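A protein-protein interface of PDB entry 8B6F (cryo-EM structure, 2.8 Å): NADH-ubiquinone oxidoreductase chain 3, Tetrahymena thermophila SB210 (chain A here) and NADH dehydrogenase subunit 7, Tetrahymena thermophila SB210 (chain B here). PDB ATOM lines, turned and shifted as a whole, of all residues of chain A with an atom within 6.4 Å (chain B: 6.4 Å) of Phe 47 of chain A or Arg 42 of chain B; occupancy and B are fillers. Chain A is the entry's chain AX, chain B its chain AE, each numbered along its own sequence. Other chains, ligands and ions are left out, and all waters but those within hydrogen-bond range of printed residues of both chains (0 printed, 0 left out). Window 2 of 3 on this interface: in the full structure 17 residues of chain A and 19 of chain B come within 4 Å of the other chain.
N of Asn 29 of chain B sits at hydrogen-bond distance from OE2 of Glu 44 of chain A, at 3.4 Å.
The backbone carbonyl oxygen (O) of Arg 42 of chain B is in hydrogen-bond range of the backbone NH (N) of His 58 of chain B (2.9 Å).
OD1 of Asn 29 of chain B lies within hydrogen-bond range of NE of Arg 42 of chain B, at 3.2 Å.
O of Asn 29 of chain B touches CB of Cys 45 of chain A, at 3.7 Å.
Cys 45 of chain A touches Gly 31 of chain B.
Cys 45 of chain A touches Pro 32 of chain B (O to CD, 3.4 Å).
Phe 47 of chain A touches Pro 32 of chain B (CE2 to CD, 3.6 Å).
CE1 of Phe 47 of chain A touches NH1 of Arg 42 of chain B, at 3.3 Å.
Phe 47 of chain A touches just these residues of chain B: Pro 32 and Arg 42.
Arg 42 of chain B touches one residue of chain A.
Printed residues of chain B within 4 Å of Glu 44 of chain A: Asn 29 (3.4 Å).
Printed residues of chain B within 4 Å of Cys 45 of chain A: Asn 29, Gly 31 and Pro 32.
Printed residues of chain A within 4 Å of Asn 29 of chain B: Glu 44 (3.4 Å) and Cys 45 (3.7 Å).
Of the printed residues of chain A, Pro 32 of chain B touches Cys 45 (3.4 Å) and Phe 47 (3.6 Å).
The nearest residue of chain A that does not touch Arg 42 of chain B is Lys 48 of chain A (5.2 Å).
The nearest printed residue of chain A that does not touch Pro 32 of chain B is Gly 46 of chain A (5.5 Å).
Of the 9 printed residues of chain A, 3 touch a printed residue of chain B.
Printed residues of chain A that touch a printed residue of chain B: Glu 44, Cys 45 and Phe 47.
Hydrophobic or aromatic side chains of chain A that line the printed part of chain B: Phe 47.
Of the 15 printed residues of chain B, 4 touch a printed residue of chain A.
Hydrophobic or aromatic side chains of chain B that line the printed part of chain A: Pro 32.
Among the printed residues, 6 pairs touch across the chains.
Among the printed residues, no Asp or Glu carboxylate lies within 4 Å of a Lys or Arg side-chain nitrogen of the other chain.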
ATOM      1  N   PHE A  42     -15.161 -21.727  22.095  1.00  0.00           N
ATOM      2  CA  PHE A  42     -14.527 -22.653  21.168  1.00  0.00           C
ATOM      3  C   PHE A  42     -14.846 -22.274  19.726  1.00  0.00           C
ATOM      4  O   PHE A  42     -15.974 -21.899  19.398  1.00  0.00           O
ATOM      5  CB  PHE A  42     -14.985 -24.083  21.449  1.00  0.00           C
ATOM      6  CG  PHE A  42     -14.662 -24.558  22.833  1.00  0.00           C
ATOM      7  CD1 PHE A  42     -13.349 -24.629  23.265  1.00  0.00           C
ATOM      8  CD2 PHE A  42     -15.670 -24.950  23.697  1.00  0.00           C
ATOM      9  CE1 PHE A  42     -13.047 -25.069  24.537  1.00  0.00           C
ATOM     10  CE2 PHE A  42     -15.376 -25.391  24.970  1.00  0.00           C
ATOM     11  CZ  PHE A  42     -14.062 -25.452  25.391  1.00  0.00           C
ATOM     12  N   TYR A  43     -13.839 -22.382  18.865  1.00  0.00           N
ATOM     13  CA  TYR A  43     -13.976 -22.055  17.452  1.00  0.00           C
ATOM     14  C   TYR A  43     -14.373 -23.308  16.680  1.00  0.00           C
ATOM     15  O   TYR A  43     -13.683 -24.330  16.747  1.00  0.00           O
ATOM     16  CB  TYR A  43     -12.668 -21.477  16.914  1.00  0.00           C
ATOM     17  CG  TYR A  43     -12.554 -21.515  15.409  1.00  0.00           C
ATOM     18  CD1 TYR A  43     -13.164 -20.549  14.623  1.00  0.00           C
ATOM     19  CD2 TYR A  43     -11.829 -22.514  14.776  1.00  0.00           C
ATOM     20  CE1 TYR A  43     -13.058 -20.579  13.248  1.00  0.00           C
ATOM     21  CE2 TYR A  43     -11.718 -22.553  13.404  1.00  0.00           C
ATOM     22  CZ  TYR A  43     -12.333 -21.583  12.646  1.00  0.00           C
ATOM     23  OH  TYR A  43     -12.225 -21.620  11.275  1.00  0.00           O
ATOM     24  N   GLU A  44     -15.481 -23.225  15.947  1.00  0.00           N
ATOM     25  CA  GLU A  44     -16.010 -24.329  15.151  1.00  0.00           C
ATOM     26  C   GLU A  44     -16.398 -23.836  13.764  1.00  0.00           C
ATOM     27  O   GLU A  44     -17.494 -24.094  13.264  1.00  0.00           O
ATOM     28  CB  GLU A  44     -17.203 -24.976  15.849  1.00  0.00           C
ATOM     29  CG  GLU A  44     -17.638 -26.309  15.255  1.00  0.00           C
ATOM     30  CD  GLU A  44     -16.670 -27.434  15.559  1.00  0.00           C
ATOM     31  OE1 GLU A  44     -15.644 -27.178  16.222  1.00  0.00           O
ATOM     32  OE2 GLU A  44     -16.939 -28.577  15.135  1.00  0.00           O
ATOM     33  N   CYS A  45     -15.493 -23.090  13.130  1.00  0.00           N
ATOM     34  CA  CYS A  45     -15.696 -22.583  11.773  1.00  0.00           C
ATOM     35  C   CYS A  45     -16.858 -21.591  11.720  1.00  0.00           C
ATOM     36  O   CYS A  45     -17.720 -21.654  10.844  1.00  0.00           O
ATOM     37  CB  CYS A  45     -15.916 -23.731  10.783  1.00  0.00           C
ATOM     38  SG  CYS A  45     -14.517 -24.858  10.615  1.00  0.00           S
ATOM     39  N   GLY A  46     -16.874 -20.664  12.674  1.00  0.00           N
ATOM     40  CA  GLY A  46     -17.849 -19.593  12.648  1.00  0.00           C
ATOM     41  C   GLY A  46     -19.205 -19.935  13.215  1.00  0.00           C
ATOM     42  O   GLY A  46     -20.179 -19.240  12.913  1.00  0.00           O
ATOM     43  N   PHE A  47     -19.310 -20.985  14.024  1.00  0.00           N
ATOM     44  CA  PHE A  47     -20.565 -21.319  14.677  1.00  0.00           C
ATOM     45  C   PHE A  47     -20.260 -21.969  16.016  1.00  0.00           C
ATOM     46  O   PHE A  47     -19.161 -22.476  16.245  1.00  0.00           O
ATOM     47  CB  PHE A  47     -21.429 -22.238  13.804  1.00  0.00           C
ATOM     48  CG  PHE A  47     -22.159 -21.516  12.707  1.00  0.00           C
ATOM     49  CD1 PHE A  47     -23.371 -20.894  12.957  1.00  0.00           C
ATOM     50  CD2 PHE A  47     -21.634 -21.458  11.427  1.00  0.00           C
ATOM     51  CE1 PHE A  47     -24.049 -20.226  11.951  1.00  0.00           C
ATOM     52  CE2 PHE A  47     -22.306 -20.793  10.417  1.00  0.00           C
ATOM     53  CZ  PHE A  47     -23.515 -20.175  10.681  1.00  0.00           C
ATOM     54  N   LYS A  48     -21.245 -21.937  16.907  1.00  0.00           N
ATOM     55  CA  LYS A  48     -21.042 -22.455  18.251  1.00  0.00           C
ATOM     56  C   LYS A  48     -20.893 -23.971  18.221  1.00  0.00           C
ATOM     57  O   LYS A  48     -21.636 -24.671  17.530  1.00  0.00           O
ATOM     58  CB  LYS A  48     -22.207 -22.055  19.153  1.00  0.00           C
ATOM     59  CG  LYS A  48     -21.968 -22.325  20.626  1.00  0.00           C
ATOM     60  CD  LYS A  48     -23.017 -21.644  21.486  1.00  0.00           C
ATOM     61  CE  LYS A  48     -22.767 -21.893  22.962  1.00  0.00           C
ATOM     62  NZ  LYS A  48     -23.766 -21.198  23.823  1.00  0.00           N
ATOM     63  N   SER A  49     -19.923 -24.477  18.979  1.00  0.00           N
ATOM     64  CA  SER A  49     -19.698 -25.912  19.070  1.00  0.00           C
ATOM     65  C   SER A  49     -20.741 -26.537  19.985  1.00  0.00           C
ATOM     66  O   SER A  49     -20.942 -26.083  21.115  1.00  0.00           O
ATOM     67  CB  SER A  49     -18.291 -26.202  19.591  1.00  0.00           C
ATOM     68  OG  SER A  49     -18.083 -25.595  20.853  1.00  0.00           O
ATOM     69  N   ILE A  50     -21.405 -27.585  19.496  1.00  0.00           N
ATOM     70  CA  ILE A  50     -22.490 -28.186  20.264  1.00  0.00           C
ATOM     71  C   ILE A  50     -21.943 -28.924  21.479  1.00  0.00           C
ATOM     72  O   ILE A  50     -22.523 -28.860  22.570  1.00  0.00           O
ATOM     73  CB  ILE A  50     -23.342 -29.108  19.372  1.00  0.00           C
ATOM     74  CG1 ILE A  50     -22.541 -30.338  18.931  1.00  0.00           C
ATOM     75  CG2 ILE A  50     -23.859 -28.330  18.167  1.00  0.00           C
ATOM     76  CD1 ILE A  50     -23.297 -31.271  18.015  1.00  0.00           C
ATOM     77  N   ASN B  29     -18.889 -29.232  12.372  1.00  0.00           N
ATOM     78  CA  ASN B  29     -19.473 -28.265  11.444  1.00  0.00           C
ATOM     79  C   ASN B  29     -18.438 -27.969  10.365  1.00  0.00           C
ATOM     80  O   ASN B  29     -17.727 -26.966  10.398  1.00  0.00           O
ATOM     81  CB  ASN B  29     -19.899 -26.995  12.172  1.00  0.00           C
ATOM     82  CG  ASN B  29     -21.135 -27.193  13.021  1.00  0.00           C
ATOM     83  OD1 ASN B  29     -22.249 -26.905  12.587  1.00  0.00           O
ATOM     84  ND2 ASN B  29     -20.947 -27.687  14.238  1.00  0.00           N
ATOM     85  N   PHE B  30     -18.352 -28.874   9.393  1.00  0.00           N
ATOM     86  CA  PHE B  30     -17.475 -28.660   8.250  1.00  0.00           C
ATOM     87  C   PHE B  30     -17.927 -27.407   7.511  1.00  0.00           C
ATOM     88  O   PHE B  30     -18.997 -27.394   6.898  1.00  0.00           O
ATOM     89  CB  PHE B  30     -17.501 -29.888   7.337  1.00  0.00           C
ATOM     90  CG  PHE B  30     -16.588 -29.791   6.152  1.00  0.00           C
ATOM     91  CD1 PHE B  30     -15.266 -30.192   6.245  1.00  0.00           C
ATOM     92  CD2 PHE B  30     -17.058 -29.320   4.937  1.00  0.00           C
ATOM     93  CE1 PHE B  30     -14.425 -30.112   5.152  1.00  0.00           C
ATOM     94  CE2 PHE B  30     -16.222 -29.237   3.839  1.00  0.00           C
ATOM     95  CZ  PHE B  30     -14.905 -29.635   3.946  1.00  0.00           C
ATOM     96  N   GLY B  31     -17.114 -26.355   7.557  1.00  0.00           N
ATOM     97  CA  GLY B  31     -17.506 -25.073   7.029  1.00  0.00           C
ATOM     98  C   GLY B  31     -18.421 -24.334   7.985  1.00  0.00           C
ATOM     99  O   GLY B  31     -18.686 -24.789   9.101  1.00  0.00           O
ATOM    100  N   PRO B  32     -18.925 -23.168   7.563  1.00  0.00           N
ATOM    101  CA  PRO B  32     -18.665 -22.503   6.277  1.00  0.00           C
ATOM    102  C   PRO B  32     -17.245 -21.970   6.168  1.00  0.00           C
ATOM    103  O   PRO B  32     -16.648 -22.002   5.099  1.00  0.00           O
ATOM    104  CB  PRO B  32     -19.691 -21.362   6.265  1.00  0.00           C
ATOM    105  CG  PRO B  32     -19.978 -21.088   7.708  1.00  0.00           C
ATOM    106  CD  PRO B  32     -19.896 -22.424   8.383  1.00  0.00           C
ATOM    107  N   ALA B  37     -14.133 -26.305   2.385  1.00  0.00           N
ATOM    108  CA  ALA B  37     -15.444 -25.826   1.976  1.00  0.00           C
ATOM    109  C   ALA B  37     -15.306 -24.530   1.189  1.00  0.00           C
ATOM    110  O   ALA B  37     -14.460 -23.685   1.496  1.00  0.00           O
ATOM    111  CB  ALA B  37     -16.338 -25.610   3.195  1.00  0.00           C
ATOM    112  N   VAL B  40     -19.646 -21.296   1.947  1.00  0.00           N
ATOM    113  CA  VAL B  40     -21.041 -21.113   2.330  1.00  0.00           C
ATOM    114  C   VAL B  40     -21.712 -22.464   2.532  1.00  0.00           C
ATOM    115  O   VAL B  40     -22.938 -22.580   2.429  1.00  0.00           O
ATOM    116  CB  VAL B  40     -21.789 -20.275   1.281  1.00  0.00           C
ATOM    117  CG1 VAL B  40     -21.249 -18.863   1.269  1.00  0.00           C
ATOM    118  CG2 VAL B  40     -21.661 -20.908  -0.096  1.00  0.00           C
ATOM    119  N   LEU B  41     -20.921 -23.492   2.820  1.00  0.00           N
ATOM    120  CA  LEU B  41     -21.437 -24.827   3.086  1.00  0.00           C
ATOM    121  C   LEU B  41     -21.272 -25.122   4.568  1.00  0.00           C
ATOM    122  O   LEU B  41     -20.153 -25.083   5.088  1.00  0.00           O
ATOM    123  CB  LEU B  41     -20.703 -25.875   2.251  1.00  0.00           C
ATOM    124  CG  LEU B  41     -21.126 -27.331   2.472  1.00  0.00           C
ATOM    125  CD1 LEU B  41     -22.575 -27.543   2.070  1.00  0.00           C
ATOM    126  CD2 LEU B  41     -20.215 -28.285   1.718  1.00  0.00           C
ATOM    127  N   ARG B  42     -22.377 -25.411   5.242  1.00  0.00           N
ATOM    128  CA  ARG B  42     -22.355 -25.818   6.641  1.00  0.00           C
ATOM    129  C   ARG B  42     -22.772 -27.283   6.673  1.00  0.00           C
ATOM    130  O   ARG B  42     -23.952 -27.608   6.796  1.00  0.00           O
ATOM    131  CB  ARG B  42     -23.274 -24.950   7.487  1.00  0.00           C
ATOM    132  CG  ARG B  42     -23.223 -25.274   8.967  1.00  0.00           C
ATOM    133  CD  ARG B  42     -24.144 -24.371   9.765  1.00  0.00           C
ATOM    134  NE  ARG B  42     -24.139 -24.718  11.180  1.00  0.00           N
ATOM    135  CZ  ARG B  42     -24.859 -24.104  12.106  1.00  0.00           C
ATOM    136  NH1 ARG B  42     -25.664 -23.099  11.803  1.00  0.00           N
ATOM    137  NH2 ARG B  42     -24.769 -24.507  13.369  1.00  0.00           N
ATOM    138  N   LEU B  43     -21.789 -28.167   6.544  1.00  0.00           N
ATOM    139  CA  LEU B  43     -22.034 -29.604   6.506  1.00  0.00           C
ATOM    140  C   LEU B  43     -21.860 -30.151   7.916  1.00  0.00           C
ATOM    141  O   LEU B  43     -20.753 -30.128   8.463  1.00  0.00           O
ATOM    142  CB  LEU B  43     -21.082 -30.277   5.520  1.00  0.00           C
ATOM    143  CG  LEU B  43     -21.161 -31.800   5.398  1.00  0.00           C
ATOM    144  CD1 LEU B  43     -22.473 -32.220   4.766  1.00  0.00           C
ATOM    145  CD2 LEU B  43     -19.988 -32.326   4.596  1.00  0.00           C
ATOM    146  N   ILE B  44     -22.945 -30.639   8.509  1.00  0.00           N
ATOM    147  CA  ILE B  44     -22.857 -31.349   9.780  1.00  0.00           C
ATOM    148  C   ILE B  44     -22.388 -32.765   9.471  1.00  0.00           C
ATOM    149  O   ILE B  44     -23.120 -33.554   8.871  1.00  0.00           O
ATOM    150  CB  ILE B  44     -24.193 -31.351  10.530  1.00  0.00           C
ATOM    151  CG1 ILE B  44     -24.856 -29.971  10.462  1.00  0.00           C
ATOM    152  CG2 ILE B  44     -23.982 -31.760  11.978  1.00  0.00           C
ATOM    153  CD1 ILE B  44     -23.963 -28.830  10.914  1.00  0.00           C
ATOM    154  N   ASP B  56     -25.339 -33.966   6.910  1.00  0.00           N
ATOM    155  CA  ASP B  56     -26.477 -33.049   6.954  1.00  0.00           C
ATOM    156  C   ASP B  56     -25.997 -31.717   6.396  1.00  0.00           C
ATOM    157  O   ASP B  56     -25.553 -30.840   7.150  1.00  0.00           O
ATOM    158  CB  ASP B  56     -27.020 -32.901   8.372  1.00  0.00           C
ATOM    159  CG  ASP B  56     -28.361 -32.200   8.412  1.00  0.00           C
ATOM    160  OD1 ASP B  56     -28.666 -31.440   7.471  1.00  0.00           O
ATOM    161  OD2 ASP B  56     -29.109 -32.402   9.391  1.00  0.00           O
ATOM    162  N   PRO B  57     -26.070 -31.528   5.081  1.00  0.00           N
ATOM    163  CA  PRO B  57     -25.621 -30.259   4.497  1.00  0.00           C
ATOM    164  C   PRO B  57     -26.661 -29.161   4.649  1.00  0.00           C
ATOM    165  O   PRO B  57     -27.859 -29.374   4.448  1.00  0.00           O
ATOM    166  CB  PRO B  57     -25.390 -30.605   3.018  1.00  0.00           C
ATOM    167  CG  PRO B  57     -25.479 -32.100   2.926  1.00  0.00           C
ATOM    168  CD  PRO B  57     -26.355 -32.531   4.045  1.00  0.00           C
ATOM    169  N   HIS B  58     -26.183 -27.973   5.011  1.00  0.00           N
ATOM    170  CA  HIS B  58     -26.970 -26.749   4.953  1.00  0.00           C
ATOM    171  C   HIS B  58     -26.322 -25.841   3.921  1.00  0.00           C
ATOM    172  O   HIS B  58     -25.132 -25.526   4.027  1.00  0.00           O
ATOM    173  CB  HIS B  58     -27.041 -26.056   6.315  1.00  0.00           C
ATOM    174  CG  HIS B  58     -27.424 -26.965   7.440  1.00  0.00           C
ATOM    175  ND1 HIS B  58     -28.686 -27.502   7.567  1.00  0.00           N
ATOM    176  CD2 HIS B  58     -26.715 -27.421   8.498  1.00  0.00           C
ATOM    177  CE1 HIS B  58     -28.736 -28.256   8.649  1.00  0.00           C
ATOM    178  NE2 HIS B  58     -27.553 -28.224   9.234  1.00  0.00           N
ATOM    179  N   ILE B  59     -27.103 -25.423   2.927  1.00  0.00           N
ATOM    180  CA  ILE B  59     -26.599 -24.693   1.775  1.00  0.00           C
ATOM    181  C   ILE B  59     -27.257 -23.327   1.624  1.00  0.00           C
ATOM    182  O   ILE B  59     -27.068 -22.665   0.606  1.00  0.00           O
ATOM    183  CB  ILE B  59     -26.764 -25.522   0.486  1.00  0.00           C
ATOM    184  CG1 ILE B  59     -28.222 -25.960   0.330  1.00  0.00           C
ATOM    185  CG2 ILE B  59     -25.839 -26.727   0.521  1.00  0.00           C
ATOM    186  CD1 ILE B  59     -28.518 -26.682  -0.963  1.00  0.00           C
ATOM    187  N   LEU B  61     -26.566 -20.604   3.183  1.00  0.00           N
ATOM    188  CA  LEU B  61     -25.709 -19.494   3.575  1.00  0.00           C
ATOM    189  C   LEU B  61     -25.413 -18.544   2.423  1.00  0.00           C
ATOM    190  O   LEU B  61     -24.842 -17.474   2.661  1.00  0.00           O
ATOM    191  CB  LEU B  61     -24.400 -20.025   4.160  1.00  0.00           C
ATOM    192  CG  LEU B  61     -24.537 -20.983   5.348  1.00  0.00           C
ATOM    193  CD1 LEU B  61     -23.169 -21.377   5.867  1.00  0.00           C
ATOM    194  CD2 LEU B  61     -25.367 -20.373   6.462  1.00  0.00           C
